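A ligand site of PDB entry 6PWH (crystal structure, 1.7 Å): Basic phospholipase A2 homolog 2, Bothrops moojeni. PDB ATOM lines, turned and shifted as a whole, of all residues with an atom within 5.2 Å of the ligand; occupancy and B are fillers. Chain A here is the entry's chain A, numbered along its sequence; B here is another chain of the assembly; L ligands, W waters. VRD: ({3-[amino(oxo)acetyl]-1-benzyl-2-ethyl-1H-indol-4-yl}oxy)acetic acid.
The side-chain sulfur (SG) of Cys 28 is disulfide-bonded to the side-chain sulfur (SG) of Cys 44 (2.0 Å). The backbone carbonyl oxygen (O) of Lys 60 is in hydrogen-bond range of the backbone NH (N) of Leu 2 (3.0 Å). The backbone carbonyl oxygen of Asn 27 lies within hydrogen-bond range of the side-chain amino group of Lys 48. N of Val 30 sits at hydrogen-bond distance from O of Gly 22, at 3.3 Å. NE2 of His 47 sits close to OH of Tyr 51 (3.4 Å). N of Gly 22 sits at hydrogen-bond distance from O of Pro 17, at 3.5 Å. The backbone carbonyl oxygen of Gly 29 sits at hydrogen-bond distance from the side-chain amino group of Lys 48 (2.7 Å).
The backbone carbonyl oxygen (O) of Asn 27 sits close to an oxygen (O27) of the ligand (3.1 Å). O of Leu 2 touches C12 of the ligand (3.3 Å). Leu 5 touches the ligand. Gly 6 touches the ligand. Ile 9 touches the ligand (CD1 to C02, 3.7 Å). CA of Ala 18 touches C14 of the ligand, 3.5 Å away. Tyr 21 touches the ligand. Gly 22 touches the ligand. Cys 28 touches the ligand (CA to O27, 3.2 Å). Tyr 51 touches the ligand. Pro 114 of chain B touches the ligand (CG to C15, 3.99 Å). Phe 115 of chain B touches the ligand. Hydrophobic or aromatic side chains within 4 Å of the ligand: Leu 5, Ile 9, Ala 18, Tyr 21, His 47, Tyr 51, Pro 114 of chain B and Phe 115 of chain B. 16 residues have an atom within 4 Å of the ligand: Leu 2, Leu 5, Gly 6, Ile 9, Ala 18, Tyr 21, Gly 22, Asn 27, Cys 28, Gly 29, Cys 44, His 47, Lys 48, Tyr 51, Pro 114 of chain B and Phe 115 of chain B. The nearest printed residue that does not touch the ligand is Pro 17 (4.04 Å).
O of Cys 44 is in hydrogen-bond range of N28 of the ligand, at 3.1 Å. A ring nitrogen (ND1) of His 47 is in hydrogen-bond range of a nitrogen (N28) of the ligand. An oxygen (O23) of the ligand lies within salt-bridge range of the side-chain amino group (NZ) of Lys 48, at 2.8 Å. N of Gly 29 lies within hydrogen-bond range of O27 of the ligand (2.8 Å).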
ATOM      1  N   LEU A   2      19.439  -1.388  15.431  1.00  0.00           N
ATOM      2  CA  LEU A   2      20.869  -1.346  15.099  1.00  0.00           C
ATOM      3  C   LEU A   2      21.730  -1.595  16.323  1.00  0.00           C
ATOM      4  O   LEU A   2      22.883  -2.021  16.199  1.00  0.00           O
ATOM      5  CB  LEU A   2      21.218   0.000  14.463  1.00  0.00           C
ATOM      6  CG  LEU A   2      20.756   0.224  13.024  1.00  0.00           C
ATOM      7  CD1 LEU A   2      21.478   1.414  12.408  1.00  0.00           C
ATOM      8  CD2 LEU A   2      20.958  -1.031  12.171  1.00  0.00           C
ATOM      9  N   LEU A   5      21.916  -5.430  16.531  1.00  0.00           N
ATOM     10  CA  LEU A   5      22.693  -5.917  15.397  1.00  0.00           C
ATOM     11  C   LEU A   5      24.189  -5.703  15.637  1.00  0.00           C
ATOM     12  O   LEU A   5      24.995  -6.618  15.451  1.00  0.00           O
ATOM     13  CB  LEU A   5      22.244  -5.231  14.116  1.00  0.00           C
ATOM     14  CG  LEU A   5      23.076  -5.493  12.871  1.00  0.00           C
ATOM     15  CD1 LEU A   5      23.108  -6.985  12.561  1.00  0.00           C
ATOM     16  CD2 LEU A   5      22.555  -4.691  11.679  1.00  0.00           C
ATOM     17  N   GLY A   6      24.570  -4.491  16.044  1.00  0.00           N
ATOM     18  CA  GLY A   6      25.981  -4.207  16.294  1.00  0.00           C
ATOM     19  C   GLY A   6      26.561  -5.058  17.409  1.00  0.00           C
ATOM     20  O   GLY A   6      27.724  -5.463  17.351  1.00  0.00           O
ATOM     21  N   ILE A   9      27.329  -8.470  15.890  1.00  0.00           N
ATOM     22  CA  ILE A   9      28.465  -8.434  14.986  1.00  0.00           C
ATOM     23  C   ILE A   9      29.769  -8.328  15.772  1.00  0.00           C
ATOM     24  O   ILE A   9      30.763  -8.973  15.443  1.00  0.00           O
ATOM     25  CB  ILE A   9      28.306  -7.269  13.988  1.00  0.00           C
ATOM     26  CG1 ILE A   9      27.132  -7.546  13.048  1.00  0.00           C
ATOM     27  CG2 ILE A   9      29.598  -7.065  13.199  1.00  0.00           C
ATOM     28  CD1 ILE A   9      26.780  -6.387  12.132  1.00  0.00           C
ATOM     29  N   PRO A  17      31.641  -2.928  14.533  1.00  0.00           N
ATOM     30  CA  PRO A  17      30.724  -3.132  13.398  1.00  0.00           C
ATOM     31  C   PRO A  17      30.590  -1.915  12.497  1.00  0.00           C
ATOM     32  O   PRO A  17      30.585  -2.064  11.264  1.00  0.00           O
ATOM     33  CB  PRO A  17      29.388  -3.487  14.072  1.00  0.00           C
ATOM     34  CG  PRO A  17      29.524  -3.090  15.503  1.00  0.00           C
ATOM     35  CD  PRO A  17      30.975  -3.072  15.843  1.00  0.00           C
ATOM     36  N   ALA A  18      30.484  -0.714  13.068  1.00  0.00           N
ATOM     37  CA  ALA A  18      30.306   0.478  12.245  1.00  0.00           C
ATOM     38  C   ALA A  18      31.561   0.767  11.423  1.00  0.00           C
ATOM     39  O   ALA A  18      31.470   1.021  10.221  1.00  0.00           O
ATOM     40  CB  ALA A  18      29.951   1.675  13.126  1.00  0.00           C
ATOM     41  N   TYR A  21      32.205  -2.338   8.827  1.00  0.00           N
ATOM     42  CA  TYR A  21      31.155  -2.733   7.898  1.00  0.00           C
ATOM     43  C   TYR A  21      30.175  -1.617   7.545  1.00  0.00           C
ATOM     44  O   TYR A  21      29.355  -1.821   6.651  1.00  0.00           O
ATOM     45  CB  TYR A  21      30.358  -3.913   8.468  1.00  0.00           C
ATOM     46  CG  TYR A  21      31.170  -5.149   8.755  1.00  0.00           C
ATOM     47  CD1 TYR A  21      31.620  -5.966   7.728  1.00  0.00           C
ATOM     48  CD2 TYR A  21      31.476  -5.516  10.059  1.00  0.00           C
ATOM     49  CE1 TYR A  21      32.366  -7.114   7.985  1.00  0.00           C
ATOM     50  CE2 TYR A  21      32.214  -6.657  10.336  1.00  0.00           C
ATOM     51  CZ  TYR A  21      32.653  -7.448   9.292  1.00  0.00           C
ATOM     52  OH  TYR A  21      33.382  -8.579   9.567  1.00  0.00           O
ATOM     53  N   GLY A  22      30.227  -0.463   8.217  1.00  0.00           N
ATOM     54  CA  GLY A  22      29.226   0.565   8.011  1.00  0.00           C
ATOM     55  C   GLY A  22      29.200   1.161   6.606  1.00  0.00           C
ATOM     56  O   GLY A  22      28.184   1.741   6.218  1.00  0.00           O
ATOM     57  N   ASN A  27      26.940  -3.251  -0.411  1.00  0.00           N
ATOM     58  CA  ASN A  27      25.727  -3.647   0.313  1.00  0.00           C
ATOM     59  C   ASN A  27      25.768  -3.411   1.819  1.00  0.00           C
ATOM     60  O   ASN A  27      24.700  -3.336   2.425  1.00  0.00           O
ATOM     61  CB  ASN A  27      25.433  -5.143   0.079  1.00  0.00           C
ATOM     62  CG  ASN A  27      25.044  -5.422  -1.346  1.00  0.00           C
ATOM     63  OD1 ASN A  27      23.883  -5.303  -1.715  1.00  0.00           O
ATOM     64  ND2 ASN A  27      26.025  -5.812  -2.157  1.00  0.00           N
ATOM     65  N   CYS A  28      26.944  -3.284   2.426  1.00  0.00           N
ATOM     66  CA  CYS A  28      27.011  -3.170   3.883  1.00  0.00           C
ATOM     67  C   CYS A  28      26.788  -1.724   4.318  1.00  0.00           C
ATOM     68  O   CYS A  28      27.389  -0.795   3.792  1.00  0.00           O
ATOM     69  CB  CYS A  28      28.359  -3.672   4.393  1.00  0.00           C
ATOM     70  SG  CYS A  28      28.651  -5.413   4.064  1.00  0.00           S
ATOM     71  N   GLY A  29      25.910  -1.555   5.302  1.00  0.00           N
ATOM     72  CA  GLY A  29      25.715  -0.252   5.917  1.00  0.00           C
ATOM     73  C   GLY A  29      24.812   0.664   5.120  1.00  0.00           C
ATOM     74  O   GLY A  29      23.947   0.244   4.333  1.00  0.00           O
ATOM     75  N   VAL A  30      25.019   1.969   5.341  1.00  0.00           N
ATOM     76  CA  VAL A  30      24.121   2.969   4.803  1.00  0.00           C
ATOM     77  C   VAL A  30      24.121   2.913   3.275  1.00  0.00           C
ATOM     78  O   VAL A  30      25.151   2.642   2.642  1.00  0.00           O
ATOM     79  CB  VAL A  30      24.509   4.366   5.330  1.00  0.00           C
ATOM     80  CG1 VAL A  30      25.765   4.877   4.638  1.00  0.00           C
ATOM     81  CG2 VAL A  30      23.357   5.324   5.178  1.00  0.00           C
ATOM     82  N   GLY A  31      22.968   3.162   2.693  1.00  0.00           N
ATOM     83  CA  GLY A  31      22.734   2.905   1.293  1.00  0.00           C
ATOM     84  C   GLY A  31      21.842   1.692   1.103  1.00  0.00           C
ATOM     85  O   GLY A  31      21.266   1.149   2.042  1.00  0.00           O
ATOM     86  N   CYS A  43      26.929 -11.169   2.391  1.00  0.00           N
ATOM     87  CA  CYS A  43      26.243 -11.270   3.669  1.00  0.00           C
ATOM     88  C   CYS A  43      25.309 -10.097   3.884  1.00  0.00           C
ATOM     89  O   CYS A  43      24.164 -10.253   4.321  1.00  0.00           O
ATOM     90  CB  CYS A  43      27.270 -11.341   4.814  1.00  0.00           C
ATOM     91  SG  CYS A  43      28.377 -12.748   4.777  1.00  0.00           S
ATOM     92  N   CYS A  44      25.794  -8.890   3.581  1.00  0.00           N
ATOM     93  CA  CYS A  44      24.968  -7.703   3.756  1.00  0.00           C
ATOM     94  C   CYS A  44      23.843  -7.638   2.743  1.00  0.00           C
ATOM     95  O   CYS A  44      22.768  -7.104   3.044  1.00  0.00           O
ATOM     96  CB  CYS A  44      25.842  -6.455   3.663  1.00  0.00           C
ATOM     97  SG  CYS A  44      27.089  -6.373   4.951  1.00  0.00           S
ATOM     98  N   TYR A  45      24.075  -8.148   1.531  1.00  0.00           N
ATOM     99  CA  TYR A  45      23.031  -8.223   0.520  1.00  0.00           C
ATOM    100  C   TYR A  45      21.886  -9.106   1.019  1.00  0.00           C
ATOM    101  O   TYR A  45      20.705  -8.727   0.929  1.00  0.00           O
ATOM    102  CB  TYR A  45      23.624  -8.774  -0.770  1.00  0.00           C
ATOM    103  CG  TYR A  45      22.665  -8.981  -1.920  1.00  0.00           C
ATOM    104  CD1 TYR A  45      21.844 -10.112  -1.977  1.00  0.00           C
ATOM    105  CD2 TYR A  45      22.611  -8.080  -2.974  1.00  0.00           C
ATOM    106  CE1 TYR A  45      20.977 -10.305  -3.037  1.00  0.00           C
ATOM    107  CE2 TYR A  45      21.753  -8.283  -4.032  1.00  0.00           C
ATOM    108  CZ  TYR A  45      20.936  -9.396  -4.064  1.00  0.00           C
ATOM    109  OH  TYR A  45      20.070  -9.586  -5.115  1.00  0.00           O
ATOM    110  N   HIS A  47      21.204  -9.854   4.092  1.00  0.00           N
ATOM    111  CA  HIS A  47      20.604  -9.242   5.278  1.00  0.00           C
ATOM    112  C   HIS A  47      19.631  -8.123   4.902  1.00  0.00           C
ATOM    113  O   HIS A  47      18.553  -8.022   5.490  1.00  0.00           O
ATOM    114  CB  HIS A  47      21.723  -8.719   6.189  1.00  0.00           C
ATOM    115  CG  HIS A  47      21.254  -8.105   7.463  1.00  0.00           C
ATOM    116  ND1 HIS A  47      21.273  -6.750   7.683  1.00  0.00           N
ATOM    117  CD2 HIS A  47      20.747  -8.664   8.588  1.00  0.00           C
ATOM    118  CE1 HIS A  47      20.809  -6.494   8.891  1.00  0.00           C
ATOM    119  NE2 HIS A  47      20.490  -7.639   9.470  1.00  0.00           N
ATOM    120  N   LYS A  48      19.992  -7.293   3.910  1.00  0.00           N
ATOM    121  CA  LYS A  48      19.063  -6.269   3.442  1.00  0.00           C
ATOM    122  C   LYS A  48      17.817  -6.891   2.824  1.00  0.00           C
ATOM    123  O   LYS A  48      16.704  -6.379   2.989  1.00  0.00           O
ATOM    124  CB  LYS A  48      19.765  -5.336   2.457  1.00  0.00           C
ATOM    125  CG  LYS A  48      20.579  -4.246   3.131  1.00  0.00           C
ATOM    126  CD  LYS A  48      21.455  -3.507   2.121  1.00  0.00           C
ATOM    127  CE  LYS A  48      21.738  -2.060   2.562  1.00  0.00           C
ATOM    128  NZ  LYS A  48      22.609  -2.001   3.760  1.00  0.00           N
ATOM    129  N   TYR A  51      15.622  -7.912   5.636  1.00  0.00           N
ATOM    130  CA  TYR A  51      14.883  -6.791   6.202  1.00  0.00           C
ATOM    131  C   TYR A  51      13.670  -6.425   5.358  1.00  0.00           C
ATOM    132  O   TYR A  51      12.656  -5.951   5.903  1.00  0.00           O
ATOM    133  CB  TYR A  51      15.801  -5.582   6.348  1.00  0.00           C
ATOM    134  CG  TYR A  51      16.583  -5.511   7.639  1.00  0.00           C
ATOM    135  CD1 TYR A  51      16.680  -6.608   8.485  1.00  0.00           C
ATOM    136  CD2 TYR A  51      17.221  -4.339   8.025  1.00  0.00           C
ATOM    137  CE1 TYR A  51      17.399  -6.537   9.668  1.00  0.00           C
ATOM    138  CE2 TYR A  51      17.931  -4.258   9.206  1.00  0.00           C
ATOM    139  CZ  TYR A  51      18.014  -5.363  10.025  1.00  0.00           C
ATOM    140  OH  TYR A  51      18.725  -5.272  11.203  1.00  0.00           O
ATOM    141  N   LYS A  60      15.481  -0.912  11.914  1.00  0.00           N
ATOM    142  CA  LYS A  60      16.570  -0.078  12.421  1.00  0.00           C
ATOM    143  C   LYS A  60      16.309   0.408  13.846  1.00  0.00           C
ATOM    144  O   LYS A  60      17.253   0.549  14.627  1.00  0.00           O
ATOM    145  CB  LYS A  60      16.784   1.116  11.492  1.00  0.00           C
ATOM    146  CG  LYS A  60      17.291   0.740  10.115  1.00  0.00           C
ATOM    147  N   VAL A  92      23.348 -12.503   9.745  1.00  0.00           N
ATOM    148  CA  VAL A  92      24.392 -11.707   9.127  1.00  0.00           C
ATOM    149  C   VAL A  92      25.641 -11.664  10.005  1.00  0.00           C
ATOM    150  O   VAL A  92      26.767 -11.674   9.508  1.00  0.00           O
ATOM    151  CB  VAL A  92      23.879 -10.294   8.775  1.00  0.00           C
ATOM    152  CG1 VAL A  92      23.749  -9.440  10.022  1.00  0.00           C
ATOM    153  CG2 VAL A  92      24.789  -9.631   7.764  1.00  0.00           C
ATOM    154  N   LEU A  96      29.184 -12.738   8.561  1.00  0.00           N
ATOM    155  CA  LEU A  96      30.350 -11.875   8.552  1.00  0.00           C
ATOM    156  C   LEU A  96      31.540 -12.550   9.223  1.00  0.00           C
ATOM    157  O   LEU A  96      32.671 -12.481   8.710  1.00  0.00           O
ATOM    158  CB  LEU A  96      30.035 -10.550   9.250  1.00  0.00           C
ATOM    159  CG  LEU A  96      28.980  -9.724   8.513  1.00  0.00           C
ATOM    160  CD1 LEU A  96      28.659  -8.434   9.265  1.00  0.00           C
ATOM    161  CD2 LEU A  96      29.443  -9.439   7.089  1.00  0.00           C
ATOM    162  N   PRO B 114      24.152   6.219  10.257  1.00  0.00           N
ATOM    163  CA  PRO B 114      22.821   5.871  10.790  1.00  0.00           C
ATOM    164  C   PRO B 114      22.636   6.240  12.253  1.00  0.00           C
ATOM    165  O   PRO B 114      21.498   6.254  12.729  1.00  0.00           O
ATOM    166  CB  PRO B 114      22.731   4.357  10.589  1.00  0.00           C
ATOM    167  CG  PRO B 114      24.133   3.894  10.549  1.00  0.00           C
ATOM    168  CD  PRO B 114      24.930   5.008   9.937  1.00  0.00           C
ATOM    169  N   PHE B 115      23.716   6.526  12.980  1.00  0.00           N
ATOM    170  CA  PHE B 115      23.628   6.960  14.366  1.00  0.00           C
ATOM    171  C   PHE B 115      23.682   8.478  14.508  1.00  0.00           C
ATOM    172  O   PHE B 115      23.932   8.992  15.602  1.00  0.00           O
ATOM    173  CB  PHE B 115      24.748   6.319  15.194  1.00  0.00           C
ATOM    174  CG  PHE B 115      24.647   4.817  15.255  1.00  0.00           C
ATOM    175  CD1 PHE B 115      23.901   4.205  16.250  1.00  0.00           C
ATOM    176  CD2 PHE B 115      25.281   4.023  14.323  1.00  0.00           C
ATOM    177  CE1 PHE B 115      23.800   2.829  16.312  1.00  0.00           C
ATOM    178  CE2 PHE B 115      25.189   2.653  14.372  1.00  0.00           C
ATOM    179  CZ  PHE B 115      24.444   2.053  15.373  1.00  0.00           C
HETATM  180  C01 VRD L   1      26.966  -4.938   8.076  1.00  0.00           C
HETATM  181  C02 VRD L   1      26.745  -4.004   9.267  1.00  0.00           C
HETATM  182  C03 VRD L   1      25.615  -2.990   8.998  1.00  0.00           C
HETATM  183  C04 VRD L   1      24.450  -3.250   8.306  1.00  0.00           C
HETATM  184  C05 VRD L   1      23.704  -2.072   8.304  1.00  0.00           C
HETATM  185  C06 VRD L   1      24.447  -1.151   9.000  1.00  0.00           C
HETATM  186  C08 VRD L   1      26.648  -1.111  10.185  1.00  0.00           C
HETATM  187  C09 VRD L   1      26.272  -1.174  11.684  1.00  0.00           C
HETATM  188  C10 VRD L   1      25.320  -2.076  12.122  1.00  0.00           C
HETATM  189  C11 VRD L   1      24.977  -2.131  13.456  1.00  0.00           C
HETATM  190  C12 VRD L   1      25.575  -1.285  14.354  1.00  0.00           C
HETATM  191  C13 VRD L   1      26.527  -0.381  13.926  1.00  0.00           C
HETATM  192  C14 VRD L   1      26.879  -0.329  12.581  1.00  0.00           C
HETATM  193  C15 VRD L   1      23.953   0.150   9.179  1.00  0.00           C
HETATM  194  C16 VRD L   1      22.723   0.513   8.645  1.00  0.00           C
HETATM  195  C17 VRD L   1      21.987  -0.425   7.933  1.00  0.00           C
HETATM  196  C18 VRD L   1      22.472  -1.712   7.761  1.00  0.00           C
HETATM  197  C20 VRD L   1      20.334  -2.563   7.261  1.00  0.00           C
HETATM  198  C21 VRD L   1      19.692  -1.739   6.152  1.00  0.00           C
HETATM  199  C24 VRD L   1      24.094  -4.574   7.656  1.00  0.00           C
HETATM  200  C26 VRD L   1      23.741  -4.577   6.180  1.00  0.00           C
HETATM  201  N07 VRD L   1      25.576  -1.740   9.408  1.00  0.00           N
HETATM  202  N28 VRD L   1      22.776  -5.510   5.676  1.00  0.00           N
HETATM  203  O19 VRD L   1      21.714  -2.664   7.035  1.00  0.00           O
HETATM  204  O22 VRD L   1      18.453  -1.631   6.093  1.00  0.00           O
HETATM  205  O23 VRD L   1      20.401  -1.172   5.304  1.00  0.00           O
HETATM  206  O25 VRD L   1      24.112  -5.584   8.273  1.00  0.00           O
HETATM  207  O27 VRD L   1      24.269  -3.809   5.471  1.00  0.00           O
HETATM  208  O   HOH W   1      27.076   2.275  10.197  1.00  0.00           O
